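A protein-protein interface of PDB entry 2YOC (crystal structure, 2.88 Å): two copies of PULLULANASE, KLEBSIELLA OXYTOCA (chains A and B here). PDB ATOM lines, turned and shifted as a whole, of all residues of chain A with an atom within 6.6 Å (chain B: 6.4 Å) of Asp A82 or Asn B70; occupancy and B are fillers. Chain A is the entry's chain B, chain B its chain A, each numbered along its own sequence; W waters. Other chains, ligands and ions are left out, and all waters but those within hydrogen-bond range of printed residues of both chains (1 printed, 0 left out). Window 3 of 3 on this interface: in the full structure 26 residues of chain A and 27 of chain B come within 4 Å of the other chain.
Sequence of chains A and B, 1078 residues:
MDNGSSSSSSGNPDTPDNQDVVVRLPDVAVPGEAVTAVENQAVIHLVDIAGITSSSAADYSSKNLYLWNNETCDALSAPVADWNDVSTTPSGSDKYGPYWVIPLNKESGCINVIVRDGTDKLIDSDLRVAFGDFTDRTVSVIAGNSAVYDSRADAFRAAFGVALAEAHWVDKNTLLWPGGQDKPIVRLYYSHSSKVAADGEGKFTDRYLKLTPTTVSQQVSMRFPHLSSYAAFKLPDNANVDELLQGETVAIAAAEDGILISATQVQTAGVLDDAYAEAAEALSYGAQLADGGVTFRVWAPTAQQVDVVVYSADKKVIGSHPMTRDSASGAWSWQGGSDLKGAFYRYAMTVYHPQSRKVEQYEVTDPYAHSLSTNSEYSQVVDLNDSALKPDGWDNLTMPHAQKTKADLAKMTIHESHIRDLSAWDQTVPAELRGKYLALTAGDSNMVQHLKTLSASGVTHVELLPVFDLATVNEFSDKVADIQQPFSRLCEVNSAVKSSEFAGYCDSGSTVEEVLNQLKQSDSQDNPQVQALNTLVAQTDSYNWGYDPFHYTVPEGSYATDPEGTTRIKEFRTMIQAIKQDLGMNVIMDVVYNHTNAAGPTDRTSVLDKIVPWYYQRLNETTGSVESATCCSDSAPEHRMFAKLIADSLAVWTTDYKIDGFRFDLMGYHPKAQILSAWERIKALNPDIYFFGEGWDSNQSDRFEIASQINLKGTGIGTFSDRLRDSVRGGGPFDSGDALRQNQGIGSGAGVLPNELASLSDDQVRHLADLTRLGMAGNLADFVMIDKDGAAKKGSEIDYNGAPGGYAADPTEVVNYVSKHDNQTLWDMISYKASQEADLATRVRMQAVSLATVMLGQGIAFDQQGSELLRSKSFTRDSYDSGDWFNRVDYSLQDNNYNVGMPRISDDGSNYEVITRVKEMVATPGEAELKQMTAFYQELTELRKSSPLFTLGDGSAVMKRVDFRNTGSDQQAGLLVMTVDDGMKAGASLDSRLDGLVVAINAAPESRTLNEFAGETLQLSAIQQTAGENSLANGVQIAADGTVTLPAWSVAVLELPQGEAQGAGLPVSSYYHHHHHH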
ATOM      1  N   TYR A  66      -1.546 -15.810 -20.609  1.00  0.00           N
ATOM      2  CA  TYR A  66      -1.861 -17.076 -21.267  1.00  0.00           C
ATOM      3  C   TYR A  66      -3.261 -16.870 -21.850  1.00  0.00           C
ATOM      4  O   TYR A  66      -4.248 -16.809 -21.105  1.00  0.00           O
ATOM      5  CB  TYR A  66      -1.780 -18.312 -20.340  1.00  0.00           C
ATOM      6  CG  TYR A  66      -2.139 -19.605 -21.052  1.00  0.00           C
ATOM      7  CD1 TYR A  66      -1.241 -20.219 -21.924  1.00  0.00           C
ATOM      8  CD2 TYR A  66      -3.385 -20.198 -20.875  1.00  0.00           C
ATOM      9  CE1 TYR A  66      -1.580 -21.391 -22.605  1.00  0.00           C
ATOM     10  CE2 TYR A  66      -3.729 -21.375 -21.544  1.00  0.00           C
ATOM     11  CZ  TYR A  66      -2.822 -21.971 -22.403  1.00  0.00           C
ATOM     12  OH  TYR A  66      -3.159 -23.137 -23.050  1.00  0.00           O
ATOM     13  N   PRO A  79      -4.387 -17.390 -30.561  1.00  0.00           N
ATOM     14  CA  PRO A  79      -3.845 -17.508 -29.201  1.00  0.00           C
ATOM     15  C   PRO A  79      -2.792 -18.612 -29.074  1.00  0.00           C
ATOM     16  O   PRO A  79      -3.002 -19.718 -29.575  1.00  0.00           O
ATOM     17  CB  PRO A  79      -5.088 -17.788 -28.357  1.00  0.00           C
ATOM     18  CG  PRO A  79      -6.067 -18.436 -29.291  1.00  0.00           C
ATOM     19  CD  PRO A  79      -5.627 -18.185 -30.712  1.00  0.00           C
ATOM     20  N   VAL A  80      -1.652 -18.312 -28.393  1.00  0.00           N
ATOM     21  CA  VAL A  80      -0.561 -19.282 -28.167  1.00  0.00           C
ATOM     22  C   VAL A  80      -1.063 -20.559 -27.434  1.00  0.00           C
ATOM     23  O   VAL A  80      -1.753 -20.462 -26.407  1.00  0.00           O
ATOM     24  CB  VAL A  80       0.777 -18.716 -27.566  1.00  0.00           C
ATOM     25  CG1 VAL A  80       1.331 -17.511 -28.338  1.00  0.00           C
ATOM     26  CG2 VAL A  80       0.679 -18.396 -26.074  1.00  0.00           C
ATOM     27  N   ALA A  81      -0.758 -21.738 -28.007  1.00  0.00           N
ATOM     28  CA  ALA A  81      -1.170 -23.033 -27.461  1.00  0.00           C
ATOM     29  C   ALA A  81      -0.344 -23.427 -26.231  1.00  0.00           C
ATOM     30  O   ALA A  81      -0.909 -23.843 -25.210  1.00  0.00           O
ATOM     31  CB  ALA A  81      -1.070 -24.108 -28.536  1.00  0.00           C
ATOM     32  N   ASP A  82       0.998 -23.290 -26.342  1.00  0.00           N
ATOM     33  CA  ASP A  82       2.000 -23.619 -25.324  1.00  0.00           C
ATOM     34  C   ASP A  82       1.779 -22.812 -24.034  1.00  0.00           C
ATOM     35  O   ASP A  82       1.737 -21.577 -24.067  1.00  0.00           O
ATOM     36  CB  ASP A  82       3.426 -23.406 -25.912  1.00  0.00           C
ATOM     37  CG  ASP A  82       4.646 -23.988 -25.189  1.00  0.00           C
ATOM     38  OD1 ASP A  82       4.469 -24.651 -24.163  1.00  0.00           O
ATOM     39  OD2 ASP A  82       5.781 -23.784 -25.676  1.00  0.00           O
ATOM     40  N   TRP A  83       1.576 -23.534 -22.909  1.00  0.00           N
ATOM     41  CA  TRP A  83       1.422 -22.955 -21.572  1.00  0.00           C
ATOM     42  C   TRP A  83       2.785 -22.421 -21.128  1.00  0.00           C
ATOM     43  O   TRP A  83       2.836 -21.386 -20.462  1.00  0.00           O
ATOM     44  CB  TRP A  83       0.870 -23.990 -20.565  1.00  0.00           C
ATOM     45  CG  TRP A  83       0.926 -23.546 -19.124  1.00  0.00           C
ATOM     46  CD1 TRP A  83       1.911 -23.818 -18.224  1.00  0.00           C
ATOM     47  CD2 TRP A  83      -0.008 -22.696 -18.451  1.00  0.00           C
ATOM     48  NE1 TRP A  83       1.643 -23.199 -17.028  1.00  0.00           N
ATOM     49  CE2 TRP A  83       0.466 -22.509 -17.137  1.00  0.00           C
ATOM     50  CE3 TRP A  83      -1.223 -22.101 -18.819  1.00  0.00           C
ATOM     51  CZ2 TRP A  83      -0.217 -21.731 -16.200  1.00  0.00           C
ATOM     52  CZ3 TRP A  83      -1.899 -21.333 -17.890  1.00  0.00           C
ATOM     53  CH2 TRP A  83      -1.395 -21.151 -16.598  1.00  0.00           C
ATOM     54  N   ASN A  84       3.889 -23.120 -21.521  1.00  0.00           N
ATOM     55  CA  ASN A  84       5.274 -22.725 -21.236  1.00  0.00           C
ATOM     56  C   ASN A  84       5.679 -21.473 -22.020  1.00  0.00           C
ATOM     57  O   ASN A  84       6.682 -20.840 -21.670  1.00  0.00           O
ATOM     58  CB  ASN A  84       6.263 -23.878 -21.467  1.00  0.00           C
ATOM     59  CG  ASN A  84       6.613 -24.664 -20.213  1.00  0.00           C
ATOM     60  OD1 ASN A  84       6.902 -24.106 -19.146  1.00  0.00           O
ATOM     61  ND2 ASN A  84       6.656 -25.986 -20.328  1.00  0.00           N
ATOM     62  N   ASP A  85       4.877 -21.092 -23.051  1.00  0.00           N
ATOM     63  CA  ASP A  85       5.100 -19.894 -23.856  1.00  0.00           C
ATOM     64  C   ASP A  85       4.835 -18.610 -23.064  1.00  0.00           C
ATOM     65  O   ASP A  85       3.684 -18.214 -22.831  1.00  0.00           O
ATOM     66  CB  ASP A  85       4.302 -19.924 -25.166  1.00  0.00           C
ATOM     67  CG  ASP A  85       4.744 -18.870 -26.155  1.00  0.00           C
ATOM     68  OD1 ASP A  85       5.854 -19.018 -26.727  1.00  0.00           O
ATOM     69  OD2 ASP A  85       4.002 -17.884 -26.333  1.00  0.00           O
ATOM     70  N   VAL A  86       5.939 -17.979 -22.649  1.00  0.00           N
ATOM     71  CA  VAL A  86       5.998 -16.724 -21.901  1.00  0.00           C
ATOM     72  C   VAL A  86       6.186 -15.557 -22.932  1.00  0.00           C
ATOM     73  O   VAL A  86       6.239 -14.388 -22.535  1.00  0.00           O
ATOM     74  CB  VAL A  86       7.120 -16.823 -20.805  1.00  0.00           C
ATOM     75  CG1 VAL A  86       7.323 -15.516 -20.039  1.00  0.00           C
ATOM     76  CG2 VAL A  86       6.834 -17.962 -19.825  1.00  0.00           C
ATOM     77  N   ARG A 116      -0.185 -13.568 -15.853  1.00  0.00           N
ATOM     78  CA  ARG A 116       0.949 -14.262 -15.230  1.00  0.00           C
ATOM     79  C   ARG A 116       2.260 -13.463 -15.150  1.00  0.00           C
ATOM     80  O   ARG A 116       2.453 -12.490 -15.871  1.00  0.00           O
ATOM     81  CB  ARG A 116       1.246 -15.577 -15.984  1.00  0.00           C
ATOM     82  CG  ARG A 116       0.119 -16.591 -16.071  1.00  0.00           C
ATOM     83  CD  ARG A 116       0.631 -17.878 -16.689  1.00  0.00           C
ATOM     84  NE  ARG A 116       0.806 -17.788 -18.143  1.00  0.00           N
ATOM     85  CZ  ARG A 116       1.635 -18.549 -18.852  1.00  0.00           C
ATOM     86  NH1 ARG A 116       2.401 -19.450 -18.249  1.00  0.00           N
ATOM     87  NH2 ARG A 116       1.719 -18.402 -20.166  1.00  0.00           N
ATOM     88  N   TRP B  68      -0.741 -31.546 -21.521  1.00  0.00           N
ATOM     89  CA  TRP B  68      -0.576 -30.879 -22.817  1.00  0.00           C
ATOM     90  C   TRP B  68       0.727 -31.206 -23.525  1.00  0.00           C
ATOM     91  O   TRP B  68       1.783 -31.294 -22.900  1.00  0.00           O
ATOM     92  CB  TRP B  68      -0.695 -29.348 -22.640  1.00  0.00           C
ATOM     93  CG  TRP B  68       0.235 -28.783 -21.596  1.00  0.00           C
ATOM     94  CD1 TRP B  68       0.161 -28.945 -20.236  1.00  0.00           C
ATOM     95  CD2 TRP B  68       1.385 -27.976 -21.840  1.00  0.00           C
ATOM     96  NE1 TRP B  68       1.209 -28.298 -19.623  1.00  0.00           N
ATOM     97  CE2 TRP B  68       1.967 -27.681 -20.582  1.00  0.00           C
ATOM     98  CE3 TRP B  68       1.977 -27.460 -23.000  1.00  0.00           C
ATOM     99  CZ2 TRP B  68       3.126 -26.916 -20.460  1.00  0.00           C
ATOM    100  CZ3 TRP B  68       3.114 -26.691 -22.876  1.00  0.00           C
ATOM    101  CH2 TRP B  68       3.680 -26.426 -21.622  1.00  0.00           C
ATOM    102  N   ASN B  69       0.646 -31.318 -24.854  1.00  0.00           N
ATOM    103  CA  ASN B  69       1.759 -31.612 -25.755  1.00  0.00           C
ATOM    104  C   ASN B  69       2.453 -30.341 -26.317  1.00  0.00           C
ATOM    105  O   ASN B  69       1.785 -29.454 -26.868  1.00  0.00           O
ATOM    106  CB  ASN B  69       1.274 -32.498 -26.912  1.00  0.00           C
ATOM    107  CG  ASN B  69       1.193 -33.972 -26.607  1.00  0.00           C
ATOM    108  OD1 ASN B  69       2.045 -34.536 -25.924  1.00  0.00           O
ATOM    109  ND2 ASN B  69       0.216 -34.649 -27.197  1.00  0.00           N
ATOM    110  N   ASN B  70       3.797 -30.275 -26.189  1.00  0.00           N
ATOM    111  CA  ASN B  70       4.613 -29.175 -26.717  1.00  0.00           C
ATOM    112  C   ASN B  70       5.904 -29.691 -27.372  1.00  0.00           C
ATOM    113  O   ASN B  70       6.241 -30.870 -27.196  1.00  0.00           O
ATOM    114  CB  ASN B  70       4.845 -28.042 -25.676  1.00  0.00           C
ATOM    115  CG  ASN B  70       6.010 -28.161 -24.696  1.00  0.00           C
ATOM    116  OD1 ASN B  70       6.562 -29.238 -24.431  1.00  0.00           O
ATOM    117  ND2 ASN B  70       6.377 -27.035 -24.095  1.00  0.00           N
ATOM    118  N   GLU B  71       6.615 -28.804 -28.127  1.00  0.00           N
ATOM    119  CA  GLU B  71       7.876 -29.065 -28.858  1.00  0.00           C
ATOM    120  C   GLU B  71       8.897 -29.855 -28.018  1.00  0.00           C
ATOM    121  O   GLU B  71       9.631 -30.683 -28.563  1.00  0.00           O
ATOM    122  CB  GLU B  71       8.514 -27.755 -29.349  1.00  0.00           C
ATOM    123  CG  GLU B  71       7.556 -26.834 -30.087  1.00  0.00           C
ATOM    124  CD  GLU B  71       7.465 -27.088 -31.580  1.00  0.00           C
ATOM    125  OE1 GLU B  71       8.437 -26.766 -32.300  1.00  0.00           O
ATOM    126  OE2 GLU B  71       6.401 -27.562 -32.039  1.00  0.00           O
ATOM    127  N   THR B  72       8.918 -29.610 -26.685  1.00  0.00           N
ATOM    128  CA  THR B  72       9.800 -30.277 -25.718  1.00  0.00           C
ATOM    129  C   THR B  72       9.225 -31.648 -25.291  1.00  0.00           C
ATOM    130  O   THR B  72       9.775 -32.683 -25.685  1.00  0.00           O
ATOM    131  CB  THR B  72      10.155 -29.323 -24.544  1.00  0.00           C
ATOM    132  OG1 THR B  72      10.563 -28.049 -25.057  1.00  0.00           O
ATOM    133  CG2 THR B  72      11.254 -29.878 -23.646  1.00  0.00           C
ATOM    134  N   CYS B  73       8.120 -31.650 -24.509  1.00  0.00           N
ATOM    135  CA  CYS B  73       7.472 -32.868 -23.992  1.00  0.00           C
ATOM    136  C   CYS B  73       6.167 -33.212 -24.734  1.00  0.00           C
ATOM    137  O   CYS B  73       5.080 -32.755 -24.356  1.00  0.00           O
ATOM    138  CB  CYS B  73       7.266 -32.778 -22.480  1.00  0.00           C
ATOM    139  SG  CYS B  73       8.802 -32.703 -21.510  1.00  0.00           S
ATOM    140  N   ASP B  74       6.290 -34.053 -25.777  1.00  0.00           N
ATOM    141  CA  ASP B  74       5.196 -34.462 -26.665  1.00  0.00           C
ATOM    142  C   ASP B  74       4.715 -35.941 -26.584  1.00  0.00           C
ATOM    143  O   ASP B  74       3.845 -36.337 -27.367  1.00  0.00           O
ATOM    144  CB  ASP B  74       5.523 -34.055 -28.124  1.00  0.00           C
ATOM    145  CG  ASP B  74       6.927 -34.381 -28.631  1.00  0.00           C
ATOM    146  OD1 ASP B  74       7.689 -35.063 -27.898  1.00  0.00           O
ATOM    147  OD2 ASP B  74       7.267 -33.952 -29.762  1.00  0.00           O
ATOM    148  N   ALA B  75       5.238 -36.735 -25.627  1.00  0.00           N
ATOM    149  CA  ALA B  75       4.895 -38.158 -25.472  1.00  0.00           C
ATOM    150  C   ALA B  75       3.443 -38.499 -25.017  1.00  0.00           C
ATOM    151  O   ALA B  75       3.064 -39.677 -25.019  1.00  0.00           O
ATOM    152  CB  ALA B  75       5.922 -38.851 -24.586  1.00  0.00           C
ATOM    153  N   LEU B  76       2.632 -37.477 -24.667  1.00  0.00           N
ATOM    154  CA  LEU B  76       1.230 -37.636 -24.233  1.00  0.00           C
ATOM    155  C   LEU B  76       0.317 -38.190 -25.340  1.00  0.00           C
ATOM    156  O   LEU B  76       0.574 -37.971 -26.528  1.00  0.00           O
ATOM    157  CB  LEU B  76       0.650 -36.289 -23.757  1.00  0.00           C
ATOM    158  CG  LEU B  76       1.212 -35.696 -22.477  1.00  0.00           C
ATOM    159  CD1 LEU B  76       2.237 -34.608 -22.754  1.00  0.00           C
ATOM    160  CD2 LEU B  76       0.123 -35.144 -21.653  1.00  0.00           C
ATOM    161  N   ASN B 112       4.287 -33.120 -20.011  1.00  0.00           N
ATOM    162  CA  ASN B 112       4.020 -31.872 -19.266  1.00  0.00           C
ATOM    163  C   ASN B 112       2.810 -32.051 -18.338  1.00  0.00           C
ATOM    164  O   ASN B 112       1.678 -32.160 -18.817  1.00  0.00           O
ATOM    165  CB  ASN B 112       3.772 -30.665 -20.195  1.00  0.00           C
ATOM    166  CG  ASN B 112       4.880 -30.331 -21.146  1.00  0.00           C
ATOM    167  OD1 ASN B 112       5.928 -29.791 -20.769  1.00  0.00           O
ATOM    168  ND2 ASN B 112       4.623 -30.572 -22.421  1.00  0.00           N
ATOM    169  N   ARG B 128       7.966 -31.636 -15.632  1.00  0.00           N
ATOM    170  CA  ARG B 128       8.410 -32.266 -16.861  1.00  0.00           C
ATOM    171  C   ARG B 128       8.968 -33.620 -16.452  1.00  0.00           C
ATOM    172  O   ARG B 128      10.042 -33.694 -15.841  1.00  0.00           O
ATOM    173  CB  ARG B 128       9.434 -31.389 -17.616  1.00  0.00           C
ATOM    174  CG  ARG B 128       8.785 -30.325 -18.511  1.00  0.00           C
ATOM    175  CD  ARG B 128       9.810 -29.568 -19.339  1.00  0.00           C
ATOM    176  NE  ARG B 128       9.192 -28.666 -20.320  1.00  0.00           N
ATOM    177  CZ  ARG B 128       9.854 -27.762 -21.039  1.00  0.00           C
ATOM    178  NH1 ARG B 128      11.168 -27.620 -20.898  1.00  0.00           N
ATOM    179  NH2 ARG B 128       9.207 -26.988 -21.902  1.00  0.00           N
HETATM  180  O   HOH W   1       0.401 -26.715 -26.733  1.00  0.00           O
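Water W1 bridges the backbone carbonyl oxygen (O) of Asn B69 and the backbone NH (N) of Asp A82.
No position is printed for both chains.
Of the 7 pairs that touch across the chains among the printed residues, none has its exchanged pair printed and touching as well.
The side-chain amide nitrogen of Asn B70 sits at hydrogen-bond distance from the side-chain carboxylate of Asp A82.
ND2 of Asn A84 sits close to NH2 of Arg B128 (3.2 Å).
The backbone carbonyl oxygen (O) of Cys B73 lies within hydrogen-bond range of the side-chain amide nitrogen (ND2) of Asn B112 (3.0 Å).
The backbone NH (N) of Cys B73 is in hydrogen-bond range of the side-chain amide oxygen (OD1) of Asn B70 (2.9 Å).
ND2 of Asn B112 is in hydrogen-bond range of O of Trp B68, at 3.0 Å.
OD1 of Asn B112 lies within hydrogen-bond range of NE of Arg B128 (3.5 Å).
The backbone NH (N) of Thr B72 lies close to the side-chain amide oxygen (OD1) of Asn B70, at 3.3 Å.
The side-chain amide nitrogen (ND2) of Asn B112 is in hydrogen-bond range of the side-chain amide oxygen (OD1) of Asn B70, 3.1 Å away.
Of the printed residues of chain B, Asp A82 touches Trp B68 (2.8 Å) and Asn B70 (3.1 Å).
Printed residues of chain B within 4 Å of Trp A83: Trp B68 (3.5 Å).
Of the printed residues of chain B, Asn A84 touches Trp B68 (3.3 Å), Asn B70 (3.9 Å), Asn B112 (3.9 Å) and Arg B128 (3.2 Å).
The nearest printed residue of chain A that does not touch Arg B128 is Asp A82 (5.7 Å).
Asp A82 touches Trp B68 (OD1 to CZ3, 2.8 Å).
Trp A83 touches Trp B68 (N to CZ3, 3.5 Å).
Asn A84 touches Trp B68 (ND2 to CH2, 3.3 Å).
Asn A84 touches Asn B70.
ND2 of Asn A84 touches OD1 of Asn B112 (3.9 Å).
Of the 10 printed residues of chain A, 3 touch a printed residue of chain B.
Hydrophobic or aromatic side chains of chain A within 4 Å of the printed part of chain B: Trp A83.
Of the 11 printed residues of chain B, 4 touch a printed residue of chain A.
Hydrophobic or aromatic side chains of chain B within 4 Å of the printed part of chain A: Trp B68.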
